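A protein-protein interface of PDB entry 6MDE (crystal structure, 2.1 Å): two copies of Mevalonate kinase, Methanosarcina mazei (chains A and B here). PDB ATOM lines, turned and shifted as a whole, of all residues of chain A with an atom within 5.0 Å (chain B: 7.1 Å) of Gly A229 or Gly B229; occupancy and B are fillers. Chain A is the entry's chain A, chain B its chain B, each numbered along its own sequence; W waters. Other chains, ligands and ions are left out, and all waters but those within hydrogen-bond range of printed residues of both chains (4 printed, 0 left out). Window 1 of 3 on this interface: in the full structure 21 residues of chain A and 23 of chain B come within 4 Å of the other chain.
The side-chain carboxylate (OD2) of Asp B232 is in hydrogen-bond range of the side-chain amide nitrogen (ND2) of Asn B237, 2.7 Å away.
Of the 9 printed residues of chain A, 5 touch a printed residue of chain B. Among the printed residues, 9 pairs touch across the chains. Among the printed residues, no Asp or Glu carboxylate lies within 4 Å of a Lys or Arg side-chain nitrogen of the other chain.
Of chain A, only Gly A229 (3.1 Å), Asp A232 (3.3 Å) and Ala A233 (3.6 Å) come within 4 Å of Gly B229. Printed residues of chain B within 4 Å of Leu A230: Leu B197 and Leu B230. Of the printed residues of chain B, Val A226 touches Ala B233 (3.5 Å). Of the printed residues of chain A, Asp B232 touches Gly A229 (3.4 Å). Of the printed residues of chain A, Ala B233 touches Val A226 (3.5 Å) and Gly A229 (3.6 Å). The nearest residue of chain B that does not touch Gly A229 is Leu B230 (4.4 Å). The nearest residue of chain A that does not touch Gly B229 is Leu A230 (4.3 Å). The nearest printed residue of chain A that does not touch Leu B230 is Ala A233 (4.02 Å).
Among the printed residues, pairs that only touch across the chains: Val A226 with Ala B233 (3.5 Å), Gly A229 with Asp B232 (3.4 Å), Gly A229 with Ala B233 (3.6 Å), Leu A230 with Leu B197 (3.8 Å), Leu A230 with Leu B230 (3.6 Å), Asp A232 with Gly B229 (3.3 Å), Ala A233 with Val B226 (3.5 Å) and Ala A233 with Gly B229 (3.6 Å).
Val A226 touches Ala B233, and with the chains exchanged Ala A233 touches Val B226. Gly A229 touches its own counterpart, Gly B229. Gly A229 touches Asp B232, and with the chains exchanged Asp A232 touches Gly B229. Leu A230 touches its own counterpart, Leu B230. 9 positions are printed for both chains. Of the 9 pairs that touch across the chains among the printed residues, 8 have their exchanged pair printed and touching as well.
Water W2 lies within hydrogen-bond range of OD1 of Asp A232 (2.5 Å), O of Asn B225 (2.6 Å) and NH2 of Arg B249 (2.8 Å). Water W4 lies within hydrogen-bond range of the side-chain carboxylate (OD1) of Asp A232 (2.6 Å) and the guanidinium group (NH1) of Arg B249 (3.1 Å). Water W3 lies within hydrogen-bond range of the side-chain carboxylate (OD1) of Asp B232 (2.6 Å) and the backbone carbonyl oxygen (O) of Asn A225 (2.8 Å). Water W1 lies within hydrogen-bond range of the side-chain amide nitrogen of Asn B237, the side-chain carboxylate of Asp A232 and the side-chain carboxylate of Asp B232.
The backbone carbonyl oxygen (O) of Gly B229 lies close to the backbone carbonyl oxygen (O) of Gly A229, 3.1 Å away.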
ATOM      1  N   ASN A 225      27.747 -34.549  24.703  1.00  0.00           N
ATOM      2  CA  ASN A 225      26.603 -34.524  23.793  1.00  0.00           C
ATOM      3  C   ASN A 225      25.559 -33.527  24.264  1.00  0.00           C
ATOM      4  O   ASN A 225      24.952 -32.832  23.442  1.00  0.00           O
ATOM      5  CB  ASN A 225      25.991 -35.922  23.646  1.00  0.00           C
ATOM      6  CG  ASN A 225      26.900 -36.858  22.932  1.00  0.00           C
ATOM      7  OD1 ASN A 225      27.882 -36.438  22.315  1.00  0.00           O
ATOM      8  ND2 ASN A 225      26.597 -38.144  23.008  1.00  0.00           N
ATOM      9  N   VAL A 226      25.350 -33.430  25.584  1.00  0.00           N
ATOM     10  CA  VAL A 226      24.440 -32.415  26.103  1.00  0.00           C
ATOM     11  C   VAL A 226      24.956 -31.032  25.757  1.00  0.00           C
ATOM     12  O   VAL A 226      24.204 -30.153  25.306  1.00  0.00           O
ATOM     13  CB  VAL A 226      24.240 -32.570  27.621  1.00  0.00           C
ATOM     14  CG1 VAL A 226      23.407 -31.421  28.142  1.00  0.00           C
ATOM     15  CG2 VAL A 226      23.572 -33.901  27.972  1.00  0.00           C
ATOM     16  N   ASN A 227      26.250 -30.810  25.988  1.00  0.00           N
ATOM     17  CA  ASN A 227      26.862 -29.524  25.675  1.00  0.00           C
ATOM     18  C   ASN A 227      26.672 -29.174  24.203  1.00  0.00           C
ATOM     19  O   ASN A 227      26.423 -28.012  23.856  1.00  0.00           O
ATOM     20  CB  ASN A 227      28.346 -29.583  26.019  1.00  0.00           C
ATOM     21  CG  ASN A 227      28.961 -28.215  26.234  1.00  0.00           C
ATOM     22  OD1 ASN A 227      29.989 -28.090  26.912  1.00  0.00           O
ATOM     23  ND2 ASN A 227      28.320 -27.184  25.717  1.00  0.00           N
ATOM     24  N   GLN A 228      26.809 -30.170  23.325  1.00  0.00           N
ATOM     25  CA  GLN A 228      26.620 -29.916  21.906  1.00  0.00           C
ATOM     26  C   GLN A 228      25.225 -29.366  21.642  1.00  0.00           C
ATOM     27  O   GLN A 228      25.063 -28.416  20.866  1.00  0.00           O
ATOM     28  CB  GLN A 228      26.870 -31.192  21.105  1.00  0.00           C
ATOM     29  CG  GLN A 228      26.509 -31.060  19.596  1.00  0.00           C
ATOM     30  CD  GLN A 228      27.293 -29.950  18.896  1.00  0.00           C
ATOM     31  OE1 GLN A 228      28.379 -29.542  19.349  1.00  0.00           O
ATOM     32  NE2 GLN A 228      26.756 -29.466  17.773  1.00  0.00           N
ATOM     33  N   GLY A 229      24.206 -29.940  22.298  1.00  0.00           N
ATOM     34  CA  GLY A 229      22.855 -29.424  22.148  1.00  0.00           C
ATOM     35  C   GLY A 229      22.742 -27.961  22.529  1.00  0.00           C
ATOM     36  O   GLY A 229      22.130 -27.158  21.809  1.00  0.00           O
ATOM     37  N   LEU A 230      23.338 -27.587  23.664  1.00  0.00           N
ATOM     38  CA  LEU A 230      23.236 -26.207  24.108  1.00  0.00           C
ATOM     39  C   LEU A 230      23.949 -25.280  23.141  1.00  0.00           C
ATOM     40  O   LEU A 230      23.486 -24.160  22.882  1.00  0.00           O
ATOM     41  CB  LEU A 230      23.793 -26.064  25.524  1.00  0.00           C
ATOM     42  CG  LEU A 230      23.019 -26.946  26.496  1.00  0.00           C
ATOM     43  CD1 LEU A 230      23.718 -27.103  27.856  1.00  0.00           C
ATOM     44  CD2 LEU A 230      21.645 -26.372  26.665  1.00  0.00           C
ATOM     45  N   LEU A 231      25.064 -25.738  22.581  1.00  0.00           N
ATOM     46  CA  LEU A 231      25.739 -24.934  21.579  1.00  0.00           C
ATOM     47  C   LEU A 231      24.865 -24.779  20.338  1.00  0.00           C
ATOM     48  O   LEU A 231      24.795 -23.693  19.748  1.00  0.00           O
ATOM     49  CB  LEU A 231      27.074 -25.567  21.221  1.00  0.00           C
ATOM     50  CG  LEU A 231      28.186 -25.413  22.268  1.00  0.00           C
ATOM     51  CD1 LEU A 231      29.414 -26.147  21.755  1.00  0.00           C
ATOM     52  CD2 LEU A 231      28.528 -23.937  22.581  1.00  0.00           C
ATOM     53  N   ASP A 232      24.196 -25.865  19.927  1.00  0.00           N
ATOM     54  CA  ASP A 232      23.234 -25.774  18.832  1.00  0.00           C
ATOM     55  C   ASP A 232      22.158 -24.750  19.144  1.00  0.00           C
ATOM     56  O   ASP A 232      21.815 -23.915  18.294  1.00  0.00           O
ATOM     57  CB  ASP A 232      22.609 -27.152  18.560  1.00  0.00           C
ATOM     58  CG  ASP A 232      21.747 -27.158  17.315  1.00  0.00           C
ATOM     59  OD1 ASP A 232      20.541 -26.840  17.415  1.00  0.00           O
ATOM     60  OD2 ASP A 232      22.271 -27.490  16.233  1.00  0.00           O
ATOM     61  N   ALA A 233      21.657 -24.761  20.384  1.00  0.00           N
ATOM     62  CA  ALA A 233      20.630 -23.809  20.799  1.00  0.00           C
ATOM     63  C   ALA A 233      21.116 -22.369  20.757  1.00  0.00           C
ATOM     64  O   ALA A 233      20.308 -21.447  20.592  1.00  0.00           O
ATOM     65  CB  ALA A 233      20.145 -24.148  22.209  1.00  0.00           C
ATOM     66  N   LEU B 197      16.974 -27.108  32.123  1.00  0.00           N
ATOM     67  CA  LEU B 197      16.729 -27.153  30.683  1.00  0.00           C
ATOM     68  C   LEU B 197      15.242 -27.251  30.395  1.00  0.00           C
ATOM     69  O   LEU B 197      14.753 -26.625  29.453  1.00  0.00           O
ATOM     70  CB  LEU B 197      17.468 -28.322  30.033  1.00  0.00           C
ATOM     71  CG  LEU B 197      18.991 -28.327  30.069  1.00  0.00           C
ATOM     72  CD1 LEU B 197      19.487 -29.357  29.072  1.00  0.00           C
ATOM     73  CD2 LEU B 197      19.553 -26.941  29.760  1.00  0.00           C
ATOM     74  N   LEU B 223      13.076 -18.708  18.072  1.00  0.00           N
ATOM     75  CA  LEU B 223      12.843 -19.477  19.287  1.00  0.00           C
ATOM     76  C   LEU B 223      12.641 -20.960  18.984  1.00  0.00           C
ATOM     77  O   LEU B 223      12.971 -21.814  19.815  1.00  0.00           O
ATOM     78  CB  LEU B 223      11.641 -18.904  20.018  1.00  0.00           C
ATOM     79  CG  LEU B 223      11.970 -18.039  21.227  1.00  0.00           C
ATOM     80  CD1 LEU B 223      13.090 -17.075  20.945  1.00  0.00           C
ATOM     81  CD2 LEU B 223      10.738 -17.310  21.629  1.00  0.00           C
ATOM     82  N   MET B 224      12.102 -21.281  17.808  1.00  0.00           N
ATOM     83  CA  MET B 224      12.051 -22.671  17.381  1.00  0.00           C
ATOM     84  C   MET B 224      13.452 -23.240  17.261  1.00  0.00           C
ATOM     85  O   MET B 224      13.686 -24.397  17.604  1.00  0.00           O
ATOM     86  CB  MET B 224      11.324 -22.798  16.038  1.00  0.00           C
ATOM     87  CG  MET B 224       9.827 -22.560  16.140  1.00  0.00           C
ATOM     88  SD  MET B 224       8.959 -22.514  14.551  1.00  0.00           S
ATOM     89  CE  MET B 224       9.158 -24.176  13.933  1.00  0.00           C
ATOM     90  N   ASN B 225      14.387 -22.463  16.727  1.00  0.00           N
ATOM     91  CA  ASN B 225      15.735 -22.989  16.574  1.00  0.00           C
ATOM     92  C   ASN B 225      16.410 -23.174  17.928  1.00  0.00           C
ATOM     93  O   ASN B 225      17.189 -24.114  18.104  1.00  0.00           O
ATOM     94  CB  ASN B 225      16.563 -22.076  15.682  1.00  0.00           C
ATOM     95  CG  ASN B 225      16.005 -21.968  14.249  1.00  0.00           C
ATOM     96  OD1 ASN B 225      15.288 -22.853  13.743  1.00  0.00           O
ATOM     97  ND2 ASN B 225      16.408 -20.909  13.568  1.00  0.00           N
ATOM     98  N   VAL B 226      16.126 -22.299  18.895  1.00  0.00           N
ATOM     99  CA  VAL B 226      16.643 -22.515  20.249  1.00  0.00           C
ATOM    100  C   VAL B 226      16.022 -23.761  20.856  1.00  0.00           C
ATOM    101  O   VAL B 226      16.712 -24.563  21.493  1.00  0.00           O
ATOM    102  CB  VAL B 226      16.385 -21.298  21.162  1.00  0.00           C
ATOM    103  CG1 VAL B 226      16.892 -21.602  22.589  1.00  0.00           C
ATOM    104  CG2 VAL B 226      17.017 -20.026  20.605  1.00  0.00           C
ATOM    105  N   ASN B 227      14.696 -23.913  20.708  1.00  0.00           N
ATOM    106  CA  ASN B 227      14.004 -25.086  21.238  1.00  0.00           C
ATOM    107  C   ASN B 227      14.624 -26.365  20.695  1.00  0.00           C
ATOM    108  O   ASN B 227      14.721 -27.375  21.403  1.00  0.00           O
ATOM    109  CB  ASN B 227      12.512 -24.999  20.876  1.00  0.00           C
ATOM    110  CG  ASN B 227      11.607 -25.827  21.790  1.00  0.00           C
ATOM    111  OD1 ASN B 227      10.403 -25.542  21.903  1.00  0.00           O
ATOM    112  ND2 ASN B 227      12.155 -26.877  22.404  1.00  0.00           N
ATOM    113  N   GLN B 228      15.062 -26.332  19.437  1.00  0.00           N
ATOM    114  CA  GLN B 228      15.609 -27.528  18.794  1.00  0.00           C
ATOM    115  C   GLN B 228      16.959 -27.911  19.385  1.00  0.00           C
ATOM    116  O   GLN B 228      17.278 -29.101  19.518  1.00  0.00           O
ATOM    117  CB  GLN B 228      15.741 -27.291  17.285  1.00  0.00           C
ATOM    118  CG  GLN B 228      16.569 -28.342  16.547  1.00  0.00           C
ATOM    119  CD  GLN B 228      15.977 -29.743  16.661  1.00  0.00           C
ATOM    120  OE1 GLN B 228      14.819 -29.912  17.027  1.00  0.00           O
ATOM    121  NE2 GLN B 228      16.789 -30.751  16.387  1.00  0.00           N
ATOM    122  N   GLY B 229      17.790 -26.920  19.710  1.00  0.00           N
ATOM    123  CA  GLY B 229      19.038 -27.240  20.379  1.00  0.00           C
ATOM    124  C   GLY B 229      18.800 -27.902  21.726  1.00  0.00           C
ATOM    125  O   GLY B 229      19.496 -28.853  22.099  1.00  0.00           O
ATOM    126  N   LEU B 230      17.812 -27.409  22.471  1.00  0.00           N
ATOM    127  CA  LEU B 230      17.486 -28.025  23.752  1.00  0.00           C
ATOM    128  C   LEU B 230      16.994 -29.459  23.578  1.00  0.00           C
ATOM    129  O   LEU B 230      17.371 -30.344  24.352  1.00  0.00           O
ATOM    130  CB  LEU B 230      16.446 -27.179  24.493  1.00  0.00           C
ATOM    131  CG  LEU B 230      16.897 -25.756  24.800  1.00  0.00           C
ATOM    132  CD1 LEU B 230      15.825 -24.979  25.557  1.00  0.00           C
ATOM    133  CD2 LEU B 230      18.240 -25.736  25.567  1.00  0.00           C
ATOM    134  N   LEU B 231      16.156 -29.720  22.564  1.00  0.00           N
ATOM    135  CA  LEU B 231      15.766 -31.110  22.310  1.00  0.00           C
ATOM    136  C   LEU B 231      16.983 -31.951  21.953  1.00  0.00           C
ATOM    137  O   LEU B 231      17.115 -33.094  22.402  1.00  0.00           O
ATOM    138  CB  LEU B 231      14.701 -31.183  21.199  1.00  0.00           C
ATOM    139  CG  LEU B 231      13.382 -30.531  21.628  1.00  0.00           C
ATOM    140  CD1 LEU B 231      12.388 -30.479  20.496  1.00  0.00           C
ATOM    141  CD2 LEU B 231      12.798 -31.267  22.830  1.00  0.00           C
ATOM    142  N   ASP B 232      17.890 -31.392  21.153  1.00  0.00           N
ATOM    143  CA  ASP B 232      19.137 -32.083  20.851  1.00  0.00           C
ATOM    144  C   ASP B 232      19.930 -32.345  22.130  1.00  0.00           C
ATOM    145  O   ASP B 232      20.496 -33.430  22.308  1.00  0.00           O
ATOM    146  CB  ASP B 232      19.955 -31.252  19.857  1.00  0.00           C
ATOM    147  CG  ASP B 232      21.163 -31.996  19.337  1.00  0.00           C
ATOM    148  OD1 ASP B 232      22.215 -32.013  20.020  1.00  0.00           O
ATOM    149  OD2 ASP B 232      21.056 -32.587  18.247  1.00  0.00           O
ATOM    150  N   ALA B 233      19.944 -31.373  23.052  1.00  0.00           N
ATOM    151  CA  ALA B 233      20.623 -31.584  24.338  1.00  0.00           C
ATOM    152  C   ALA B 233      19.951 -32.684  25.160  1.00  0.00           C
ATOM    153  O   ALA B 233      20.626 -33.424  25.891  1.00  0.00           O
ATOM    154  CB  ALA B 233      20.661 -30.277  25.136  1.00  0.00           C
ATOM    155  N   LEU B 234      18.622 -32.799  25.075  1.00  0.00           N
ATOM    156  CA  LEU B 234      17.928 -33.865  25.801  1.00  0.00           C
ATOM    157  C   LEU B 234      18.125 -35.231  25.172  1.00  0.00           C
ATOM    158  O   LEU B 234      17.642 -36.224  25.725  1.00  0.00           O
ATOM    159  CB  LEU B 234      16.432 -33.568  25.896  1.00  0.00           C
ATOM    160  CG  LEU B 234      16.090 -32.378  26.787  1.00  0.00           C
ATOM    161  CD1 LEU B 234      14.617 -32.105  26.722  1.00  0.00           C
ATOM    162  CD2 LEU B 234      16.548 -32.664  28.219  1.00  0.00           C
ATOM    163  N   GLY B 235      18.788 -35.300  24.024  1.00  0.00           N
ATOM    164  CA  GLY B 235      19.123 -36.544  23.390  1.00  0.00           C
ATOM    165  C   GLY B 235      18.103 -37.086  22.404  1.00  0.00           C
ATOM    166  O   GLY B 235      18.210 -38.260  22.038  1.00  0.00           O
ATOM    167  N   ASN B 237      17.378 -35.927  19.225  1.00  0.00           N
ATOM    168  CA  ASN B 237      17.685 -35.615  17.834  1.00  0.00           C
ATOM    169  C   ASN B 237      18.488 -36.748  17.188  1.00  0.00           C
ATOM    170  O   ASN B 237      19.135 -37.549  17.871  1.00  0.00           O
ATOM    171  CB  ASN B 237      18.470 -34.304  17.749  1.00  0.00           C
ATOM    172  CG  ASN B 237      18.472 -33.709  16.359  1.00  0.00           C
ATOM    173  OD1 ASN B 237      17.507 -33.843  15.620  1.00  0.00           O
ATOM    174  ND2 ASN B 237      19.548 -33.014  16.015  1.00  0.00           N
ATOM    175  N   ARG B 249      16.320 -24.396   7.011  1.00  0.00           N
ATOM    176  CA  ARG B 249      16.804 -23.088   7.447  1.00  0.00           C
ATOM    177  C   ARG B 249      17.625 -22.419   6.361  1.00  0.00           C
ATOM    178  O   ARG B 249      17.512 -21.212   6.142  1.00  0.00           O
ATOM    179  CB  ARG B 249      17.654 -23.234   8.716  1.00  0.00           C
ATOM    180  CG  ARG B 249      16.871 -23.693   9.947  1.00  0.00           C
ATOM    181  CD  ARG B 249      17.802 -23.899  11.133  1.00  0.00           C
ATOM    182  NE  ARG B 249      17.121 -24.373  12.336  1.00  0.00           N
ATOM    183  CZ  ARG B 249      17.762 -24.971  13.336  1.00  0.00           C
ATOM    184  NH1 ARG B 249      19.068 -25.168  13.233  1.00  0.00           N
ATOM    185  NH2 ARG B 249      17.115 -25.393  14.413  1.00  0.00           N
ATOM    186  N   ALA B 256      13.059 -24.157  12.212  1.00  0.00           N
ATOM    187  CA  ALA B 256      12.831 -25.572  11.974  1.00  0.00           C
ATOM    188  C   ALA B 256      13.224 -26.338  13.220  1.00  0.00           C
ATOM    189  O   ALA B 256      14.219 -26.011  13.870  1.00  0.00           O
ATOM    190  CB  ALA B 256      13.626 -26.105  10.785  1.00  0.00           C
ATOM    191  N   LYS B 257      12.430 -27.348  13.548  1.00  0.00           N
ATOM    192  CA  LYS B 257      12.662 -28.123  14.747  1.00  0.00           C
ATOM    193  C   LYS B 257      11.919 -29.440  14.633  1.00  0.00           C
ATOM    194  O   LYS B 257      11.034 -29.621  13.783  1.00  0.00           O
ATOM    195  CB  LYS B 257      12.214 -27.379  16.007  1.00  0.00           C
ATOM    196  CG  LYS B 257      10.721 -27.077  16.062  1.00  0.00           C
ATOM    197  CD  LYS B 257      10.404 -26.260  17.320  1.00  0.00           C
ATOM    198  CE  LYS B 257      10.184 -27.144  18.556  1.00  0.00           C
ATOM    199  NZ  LYS B 257       8.951 -28.020  18.407  1.00  0.00           N
HETATM  200  O   HOH W   1      21.752 -30.669  15.526  1.00  0.00           O
HETATM  201  O   HOH W   2      18.922 -25.204  16.531  1.00  0.00           O
HETATM  202  O   HOH W   3      23.836 -33.777  21.076  1.00  0.00           O
HETATM  203  O   HOH W   4      19.426 -27.565  15.170  1.00  0.00           O
